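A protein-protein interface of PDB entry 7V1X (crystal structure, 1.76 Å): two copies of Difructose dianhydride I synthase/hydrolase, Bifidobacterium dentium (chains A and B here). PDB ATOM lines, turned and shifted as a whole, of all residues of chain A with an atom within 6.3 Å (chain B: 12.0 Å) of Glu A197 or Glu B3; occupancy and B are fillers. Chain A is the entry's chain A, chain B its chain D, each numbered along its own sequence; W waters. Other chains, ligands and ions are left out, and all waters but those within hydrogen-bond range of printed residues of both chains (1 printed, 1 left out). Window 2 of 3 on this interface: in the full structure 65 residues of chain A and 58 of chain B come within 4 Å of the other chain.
The backbone carbonyl oxygen (O) of Glu B3 sits at hydrogen-bond distance from the side-chain amino group (NZ) of Lys A15 (2.8 Å). OG1 of Thr B5 sits at hydrogen-bond distance from NZ of Lys A15 (2.9 Å). The side-chain carboxylate (OE1) of Glu B3 lies close to the side-chain carboxylate (OE1) of Glu A197 (3.3 Å). O of Pro A198 lies close to OE1 of Glu B3 (3.2 Å).
Of chain B, only Glu B3 (3.3 Å) comes within 4 Å of Glu A197. Glu B3 touches just these residues of chain A: Lys A15 (2.8 Å), Tyr A195 (3.9 Å), Glu A197 (3.3 Å), Pro A198 (3.2 Å), Leu A199 (3.8 Å) and Pro A200 (3.7 Å). No residue of chain B comes within 4 Å of Pro A51. Tyr A195 touches just these residues of chain B: Glu B3 (3.9 Å) and Ile B4 (3.3 Å). No residue of chain B comes within 4 Å of Gly A196. Leu A199 touches two residues of chain B. Pro A200 touches one residue of chain B. Of the printed residues of chain B, Lys A15 touches Glu B3 and Thr B5. Of the printed residues of chain A, Thr B5 touches Lys A15. Of the printed residues of chain A, Ile B4 touches Tyr A195 (3.3 Å) and Leu A199 (3.8 Å). Leu B7 touches none of the printed residues of chain A. The nearest residue of chain B that does not touch Glu A197 is Ile B4 (8.7 Å). The nearest printed residue of chain B that does not touch Lys A15 is Ile B4 (4.2 Å).
Among the printed residues, pairs that only touch across the chains: Tyr A195 with Ile B4, Pro A200 with Glu B3, Leu A199 with Glu B3, Leu A199 with Ile B4 and Tyr A195 with Glu B3.
Water W1 lies within hydrogen-bond range of the side-chain carboxylate (OE2) of Glu A193, the backbone NH (N) of Thr B5, the side-chain amino group (NZ) of Lys A15 and the side-chain hydroxyl (OH) of Tyr A195.
Of the 11 printed residues of chain B, 3 touch a printed residue of chain A. Hydrophobic or aromatic side chains of chain B within 4 Å of the printed part of chain A: Ile B4. Along chain B the printed residues that touch a printed residue of chain A span positions 3 to 5. Among the printed residues, 9 pairs touch across the chains.
The side-chain carboxylate of Glu A193 is in salt-bridge range of the side-chain amino group of Lys A15 (2.6 Å). The backbone NH (N) of Tyr A195 is in hydrogen-bond range of the backbone carbonyl oxygen (O) of Pro A51 (3.0 Å). The side-chain amide oxygen of Asn A169 sits at hydrogen-bond distance from the backbone NH of Leu A199. The side-chain carboxylate of Glu A193 is in hydrogen-bond range of the side-chain hydroxyl of Tyr A195 (2.7 Å). O of Tyr A195 lies within hydrogen-bond range of NH1 of Arg A443, 2.9 Å away.
No position is printed for both chains. Of the 9 pairs that touch across the chains among the printed residues, none has its exchanged pair printed and touching as well.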
ATOM      1  N   LYS A  15       4.013  36.708 -26.506  1.00  0.00           N
ATOM      2  CA  LYS A  15       4.125  35.237 -26.551  1.00  0.00           C
ATOM      3  C   LYS A  15       2.860  34.666 -25.921  1.00  0.00           C
ATOM      4  O   LYS A  15       2.458  35.115 -24.781  1.00  0.00           O
ATOM      5  CB  LYS A  15       5.419  34.790 -25.869  1.00  0.00           C
ATOM      6  CG  LYS A  15       5.767  33.332 -26.107  1.00  0.00           C
ATOM      7  CD  LYS A  15       6.676  32.734 -25.054  1.00  0.00           C
ATOM      8  CE  LYS A  15       8.052  33.348 -25.069  1.00  0.00           C
ATOM      9  NZ  LYS A  15       8.865  32.892 -23.915  1.00  0.00           N
ATOM     10  N   PRO A  51       4.830  21.237 -21.665  1.00  0.00           N
ATOM     11  CA  PRO A  51       6.069  21.992 -21.849  1.00  0.00           C
ATOM     12  C   PRO A  51       6.057  23.346 -21.120  1.00  0.00           C
ATOM     13  O   PRO A  51       5.030  23.984 -20.973  1.00  0.00           O
ATOM     14  CB  PRO A  51       6.161  22.195 -23.354  1.00  0.00           C
ATOM     15  CG  PRO A  51       4.720  22.169 -23.794  1.00  0.00           C
ATOM     16  CD  PRO A  51       4.008  21.216 -22.882  1.00  0.00           C
ATOM     17  N   ASN A 169      10.241  19.829 -21.437  1.00  0.00           N
ATOM     18  CA  ASN A 169       9.158  19.472 -22.381  1.00  0.00           C
ATOM     19  C   ASN A 169       8.074  18.710 -21.659  1.00  0.00           C
ATOM     20  O   ASN A 169       6.908  18.870 -22.052  1.00  0.00           O
ATOM     21  CB  ASN A 169       9.677  18.724 -23.606  1.00  0.00           C
ATOM     22  CG  ASN A 169       9.572  19.600 -24.830  1.00  0.00           C
ATOM     23  OD1 ASN A 169       8.677  20.443 -24.930  1.00  0.00           O
ATOM     24  ND2 ASN A 169      10.485  19.411 -25.765  1.00  0.00           N
ATOM     25  N   GLU A 193       6.741  29.707 -17.097  1.00  0.00           N
ATOM     26  CA  GLU A 193       5.696  29.896 -18.114  1.00  0.00           C
ATOM     27  C   GLU A 193       5.440  28.537 -18.774  1.00  0.00           C
ATOM     28  O   GLU A 193       6.337  27.677 -18.814  1.00  0.00           O
ATOM     29  CB  GLU A 193       5.992  31.036 -19.081  1.00  0.00           C
ATOM     30  CG  GLU A 193       7.365  31.026 -19.617  1.00  0.00           C
ATOM     31  CD  GLU A 193       7.698  32.178 -20.541  1.00  0.00           C
ATOM     32  OE1 GLU A 193       7.316  33.326 -20.270  1.00  0.00           O
ATOM     33  OE2 GLU A 193       8.364  31.899 -21.516  1.00  0.00           O
ATOM     34  N   TYR A 195       3.885  26.478 -22.155  1.00  0.00           N
ATOM     35  CA  TYR A 195       3.813  26.663 -23.621  1.00  0.00           C
ATOM     36  C   TYR A 195       2.728  25.776 -24.240  1.00  0.00           C
ATOM     37  O   TYR A 195       2.387  24.705 -23.662  1.00  0.00           O
ATOM     38  CB  TYR A 195       5.161  26.348 -24.258  1.00  0.00           C
ATOM     39  CG  TYR A 195       6.292  27.147 -23.676  1.00  0.00           C
ATOM     40  CD1 TYR A 195       6.223  28.533 -23.654  1.00  0.00           C
ATOM     41  CD2 TYR A 195       7.438  26.537 -23.192  1.00  0.00           C
ATOM     42  CE1 TYR A 195       7.234  29.302 -23.099  1.00  0.00           C
ATOM     43  CE2 TYR A 195       8.478  27.294 -22.674  1.00  0.00           C
ATOM     44  CZ  TYR A 195       8.364  28.681 -22.617  1.00  0.00           C
ATOM     45  OH  TYR A 195       9.332  29.471 -22.066  1.00  0.00           O
ATOM     46  N   GLY A 196       2.229  26.232 -25.389  1.00  0.00           N
ATOM     47  CA  GLY A 196       1.082  25.640 -26.114  1.00  0.00           C
ATOM     48  C   GLY A 196       1.549  24.604 -27.126  1.00  0.00           C
ATOM     49  O   GLY A 196       0.698  23.957 -27.710  1.00  0.00           O
ATOM     50  N   GLU A 197       2.857  24.464 -27.316  1.00  0.00           N
ATOM     51  CA  GLU A 197       3.506  23.466 -28.216  1.00  0.00           C
ATOM     52  C   GLU A 197       4.800  22.984 -27.573  1.00  0.00           C
ATOM     53  O   GLU A 197       5.409  23.716 -26.776  1.00  0.00           O
ATOM     54  CB  GLU A 197       3.923  24.049 -29.567  1.00  0.00           C
ATOM     55  CG  GLU A 197       2.939  25.012 -30.199  1.00  0.00           C
ATOM     56  CD  GLU A 197       3.648  26.124 -30.968  1.00  0.00           C
ATOM     57  OE1 GLU A 197       4.621  26.713 -30.417  1.00  0.00           O
ATOM     58  OE2 GLU A 197       3.247  26.391 -32.124  1.00  0.00           O
ATOM     59  N   PRO A 198       5.288  21.772 -27.939  1.00  0.00           N
ATOM     60  CA  PRO A 198       6.576  21.285 -27.443  1.00  0.00           C
ATOM     61  C   PRO A 198       7.738  22.221 -27.810  1.00  0.00           C
ATOM     62  O   PRO A 198       7.727  22.866 -28.806  1.00  0.00           O
ATOM     63  CB  PRO A 198       6.753  19.909 -28.111  1.00  0.00           C
ATOM     64  CG  PRO A 198       5.333  19.512 -28.471  1.00  0.00           C
ATOM     65  CD  PRO A 198       4.634  20.799 -28.828  1.00  0.00           C
ATOM     66  N   LEU A 199       8.749  22.265 -26.960  1.00  0.00           N
ATOM     67  CA  LEU A 199      10.039  22.906 -27.313  1.00  0.00           C
ATOM     68  C   LEU A 199      10.728  21.976 -28.303  1.00  0.00           C
ATOM     69  O   LEU A 199      10.429  20.790 -28.315  1.00  0.00           O
ATOM     70  CB  LEU A 199      10.845  23.075 -26.028  1.00  0.00           C
ATOM     71  CG  LEU A 199      10.205  24.023 -25.021  1.00  0.00           C
ATOM     72  CD1 LEU A 199      10.678  23.704 -23.600  1.00  0.00           C
ATOM     73  CD2 LEU A 199      10.466  25.466 -25.411  1.00  0.00           C
ATOM     74  N   PRO A 200      11.672  22.443 -29.146  1.00  0.00           N
ATOM     75  CA  PRO A 200      12.422  21.522 -30.020  1.00  0.00           C
ATOM     76  C   PRO A 200      13.117  20.438 -29.183  1.00  0.00           C
ATOM     77  O   PRO A 200      13.439  20.754 -28.068  1.00  0.00           O
ATOM     78  CB  PRO A 200      13.431  22.452 -30.685  1.00  0.00           C
ATOM     79  CG  PRO A 200      12.770  23.813 -30.637  1.00  0.00           C
ATOM     80  CD  PRO A 200      12.070  23.848 -29.295  1.00  0.00           C
ATOM     81  N   ARG A 443      -2.358  24.026 -15.714  1.00  0.00           N
ATOM     82  CA  ARG A 443      -1.896  23.401 -16.985  1.00  0.00           C
ATOM     83  C   ARG A 443      -3.133  23.088 -17.858  1.00  0.00           C
ATOM     84  O   ARG A 443      -3.132  23.404 -19.075  1.00  0.00           O
ATOM     85  CB  ARG A 443      -1.102  22.141 -16.637  1.00  0.00           C
ATOM     86  CG  ARG A 443      -0.817  21.201 -17.806  1.00  0.00           C
ATOM     87  CD  ARG A 443       0.493  21.589 -18.469  1.00  0.00           C
ATOM     88  NE  ARG A 443       0.315  22.424 -19.628  1.00  0.00           N
ATOM     89  CZ  ARG A 443       1.279  23.065 -20.273  1.00  0.00           C
ATOM     90  NH1 ARG A 443       0.987  23.729 -21.369  1.00  0.00           N
ATOM     91  NH2 ARG A 443       2.517  23.068 -19.823  1.00  0.00           N
ATOM     92  N   PHE A 446      -5.152  26.040 -19.120  1.00  0.00           N
ATOM     93  CA  PHE A 446      -4.399  26.649 -20.240  1.00  0.00           C
ATOM     94  C   PHE A 446      -4.572  25.808 -21.518  1.00  0.00           C
ATOM     95  O   PHE A 446      -4.851  26.392 -22.574  1.00  0.00           O
ATOM     96  CB  PHE A 446      -2.927  26.846 -19.867  1.00  0.00           C
ATOM     97  CG  PHE A 446      -2.058  27.327 -21.006  1.00  0.00           C
ATOM     98  CD1 PHE A 446      -2.327  28.514 -21.660  1.00  0.00           C
ATOM     99  CD2 PHE A 446      -0.956  26.589 -21.425  1.00  0.00           C
ATOM    100  CE1 PHE A 446      -1.510  28.967 -22.681  1.00  0.00           C
ATOM    101  CE2 PHE A 446      -0.129  27.051 -22.443  1.00  0.00           C
ATOM    102  CZ  PHE A 446      -0.413  28.233 -23.075  1.00  0.00           C
ATOM    103  N   GLU B   3      10.747  29.219 -28.617  1.00  0.00           N
ATOM    104  CA  GLU B   3       9.719  29.759 -27.698  1.00  0.00           C
ATOM    105  C   GLU B   3      10.366  30.213 -26.389  1.00  0.00           C
ATOM    106  O   GLU B   3       9.672  30.925 -25.665  1.00  0.00           O
ATOM    107  CB  GLU B   3       8.604  28.775 -27.333  1.00  0.00           C
ATOM    108  CG  GLU B   3       7.874  28.189 -28.518  1.00  0.00           C
ATOM    109  CD  GLU B   3       8.503  26.892 -29.007  1.00  0.00           C
ATOM    110  OE1 GLU B   3       7.744  26.014 -29.484  1.00  0.00           O
ATOM    111  OE2 GLU B   3       9.752  26.752 -28.897  1.00  0.00           O
ATOM    112  N   ILE B   4      11.608  29.833 -26.062  1.00  0.00           N
ATOM    113  CA  ILE B   4      12.280  30.488 -24.895  1.00  0.00           C
ATOM    114  C   ILE B   4      12.668  31.903 -25.360  1.00  0.00           C
ATOM    115  O   ILE B   4      13.223  31.992 -26.458  1.00  0.00           O
ATOM    116  CB  ILE B   4      13.511  29.708 -24.388  1.00  0.00           C
ATOM    117  CG1 ILE B   4      13.230  28.229 -24.118  1.00  0.00           C
ATOM    118  CG2 ILE B   4      14.075  30.381 -23.156  1.00  0.00           C
ATOM    119  CD1 ILE B   4      12.144  28.017 -23.131  1.00  0.00           C
ATOM    120  N   THR B   5      12.441  32.944 -24.550  1.00  0.00           N
ATOM    121  CA  THR B   5      12.765  34.356 -24.895  1.00  0.00           C
ATOM    122  C   THR B   5      13.673  34.982 -23.838  1.00  0.00           C
ATOM    123  O   THR B   5      13.924  34.333 -22.784  1.00  0.00           O
ATOM    124  CB  THR B   5      11.496  35.195 -25.064  1.00  0.00           C
ATOM    125  OG1 THR B   5      10.734  35.066 -23.871  1.00  0.00           O
ATOM    126  CG2 THR B   5      10.691  34.775 -26.267  1.00  0.00           C
ATOM    127  N   GLY B   6      14.156  36.200 -24.117  1.00  0.00           N
ATOM    128  CA  GLY B   6      15.016  36.976 -23.211  1.00  0.00           C
ATOM    129  C   GLY B   6      16.509  36.688 -23.355  1.00  0.00           C
ATOM    130  O   GLY B   6      16.959  35.766 -24.111  1.00  0.00           O
ATOM    131  N   LEU B   7      17.282  37.448 -22.610  1.00  0.00           N
ATOM    132  CA  LEU B   7      18.734  37.561 -22.846  1.00  0.00           C
ATOM    133  C   LEU B   7      19.454  36.241 -22.509  1.00  0.00           C
ATOM    134  O   LEU B   7      20.610  36.103 -22.942  1.00  0.00           O
ATOM    135  CB  LEU B   7      19.270  38.747 -22.040  1.00  0.00           C
ATOM    136  CG  LEU B   7      19.280  38.569 -20.530  1.00  0.00           C
ATOM    137  CD1 LEU B   7      20.561  37.894 -20.043  1.00  0.00           C
ATOM    138  CD2 LEU B   7      19.075  39.929 -19.859  1.00  0.00           C
ATOM    139  N   PHE B   8      18.839  35.293 -21.796  1.00  0.00           N
ATOM    140  CA  PHE B   8      19.516  34.015 -21.472  1.00  0.00           C
ATOM    141  C   PHE B   8      19.139  32.924 -22.484  1.00  0.00           C
ATOM    142  O   PHE B   8      19.535  31.756 -22.300  1.00  0.00           O
ATOM    143  CB  PHE B   8      19.143  33.501 -20.095  1.00  0.00           C
ATOM    144  CG  PHE B   8      19.505  34.418 -18.960  1.00  0.00           C
ATOM    145  CD1 PHE B   8      20.785  34.415 -18.448  1.00  0.00           C
ATOM    146  CD2 PHE B   8      18.530  35.169 -18.322  1.00  0.00           C
ATOM    147  CE1 PHE B   8      21.109  35.200 -17.343  1.00  0.00           C
ATOM    148  CE2 PHE B   8      18.846  35.932 -17.213  1.00  0.00           C
ATOM    149  CZ  PHE B   8      20.155  35.976 -16.756  1.00  0.00           C
ATOM    150  N   LYS B   9      18.332  33.247 -23.483  1.00  0.00           N
ATOM    151  CA  LYS B   9      17.651  32.183 -24.268  1.00  0.00           C
ATOM    152  C   LYS B   9      18.643  31.263 -24.992  1.00  0.00           C
ATOM    153  O   LYS B   9      18.338  30.050 -25.093  1.00  0.00           O
ATOM    154  CB  LYS B   9      16.617  32.781 -25.216  1.00  0.00           C
ATOM    155  CG  LYS B   9      17.164  33.550 -26.404  1.00  0.00           C
ATOM    156  CD  LYS B   9      16.054  33.795 -27.418  1.00  0.00           C
ATOM    157  CE  LYS B   9      16.112  35.150 -28.087  1.00  0.00           C
ATOM    158  NZ  LYS B   9      17.203  35.200 -29.091  1.00  0.00           N
ATOM    159  N   ASP B  10      19.800  31.755 -25.443  1.00  0.00           N
ATOM    160  CA  ASP B  10      20.714  30.940 -26.270  1.00  0.00           C
ATOM    161  C   ASP B  10      21.339  29.851 -25.400  1.00  0.00           C
ATOM    162  O   ASP B  10      21.915  28.913 -25.955  1.00  0.00           O
ATOM    163  CB  ASP B  10      21.758  31.811 -26.971  1.00  0.00           C
ATOM    164  CG  ASP B  10      21.167  32.674 -28.076  1.00  0.00           C
ATOM    165  OD1 ASP B  10      20.023  32.379 -28.497  1.00  0.00           O
ATOM    166  OD2 ASP B  10      21.817  33.655 -28.473  1.00  0.00           O
ATOM    167  N   LEU B  11      21.257  29.958 -24.076  1.00  0.00           N
ATOM    168  CA  LEU B  11      21.785  28.885 -23.215  1.00  0.00           C
ATOM    169  C   LEU B  11      20.911  27.623 -23.358  1.00  0.00           C
ATOM    170  O   LEU B  11      21.366  26.563 -22.917  1.00  0.00           O
ATOM    171  CB  LEU B  11      21.808  29.353 -21.761  1.00  0.00           C
ATOM    172  CG  LEU B  11      22.711  30.532 -21.422  1.00  0.00           C
ATOM    173  CD1 LEU B  11      22.631  30.768 -19.923  1.00  0.00           C
ATOM    174  CD2 LEU B  11      24.152  30.322 -21.860  1.00  0.00           C
ATOM    175  N   THR B  12      19.686  27.744 -23.871  1.00  0.00           N
ATOM    176  CA  THR B  12      18.722  26.616 -23.921  1.00  0.00           C
ATOM    177  C   THR B  12      18.799  25.873 -25.265  1.00  0.00           C
ATOM    178  O   THR B  12      17.908  25.012 -25.536  1.00  0.00           O
ATOM    179  CB  THR B  12      17.295  27.049 -23.631  1.00  0.00           C
ATOM    180  OG1 THR B  12      16.819  27.898 -24.670  1.00  0.00           O
ATOM    181  CG2 THR B  12      17.188  27.730 -22.279  1.00  0.00           C
ATOM    182  N   LYS B  13      19.764  26.213 -26.101  1.00  0.00           N
ATOM    183  CA  LYS B  13      19.897  25.537 -27.417  1.00  0.00           C
ATOM    184  C   LYS B  13      21.367  25.220 -27.649  1.00  0.00           C
ATOM    185  O   LYS B  13      22.218  26.025 -27.317  1.00  0.00           O
ATOM    186  CB  LYS B  13      19.162  26.324 -28.505  1.00  0.00           C
ATOM    187  CG  LYS B  13      19.833  27.579 -29.028  1.00  0.00           C
ATOM    188  CD  LYS B  13      19.523  27.851 -30.497  1.00  0.00           C
ATOM    189  CE  LYS B  13      20.398  28.953 -31.078  1.00  0.00           C
ATOM    190  NZ  LYS B  13      20.309  30.205 -30.280  1.00  0.00           N
HETATM  191  O   HOH W   1      11.062  32.491 -21.965  1.00  0.00           O
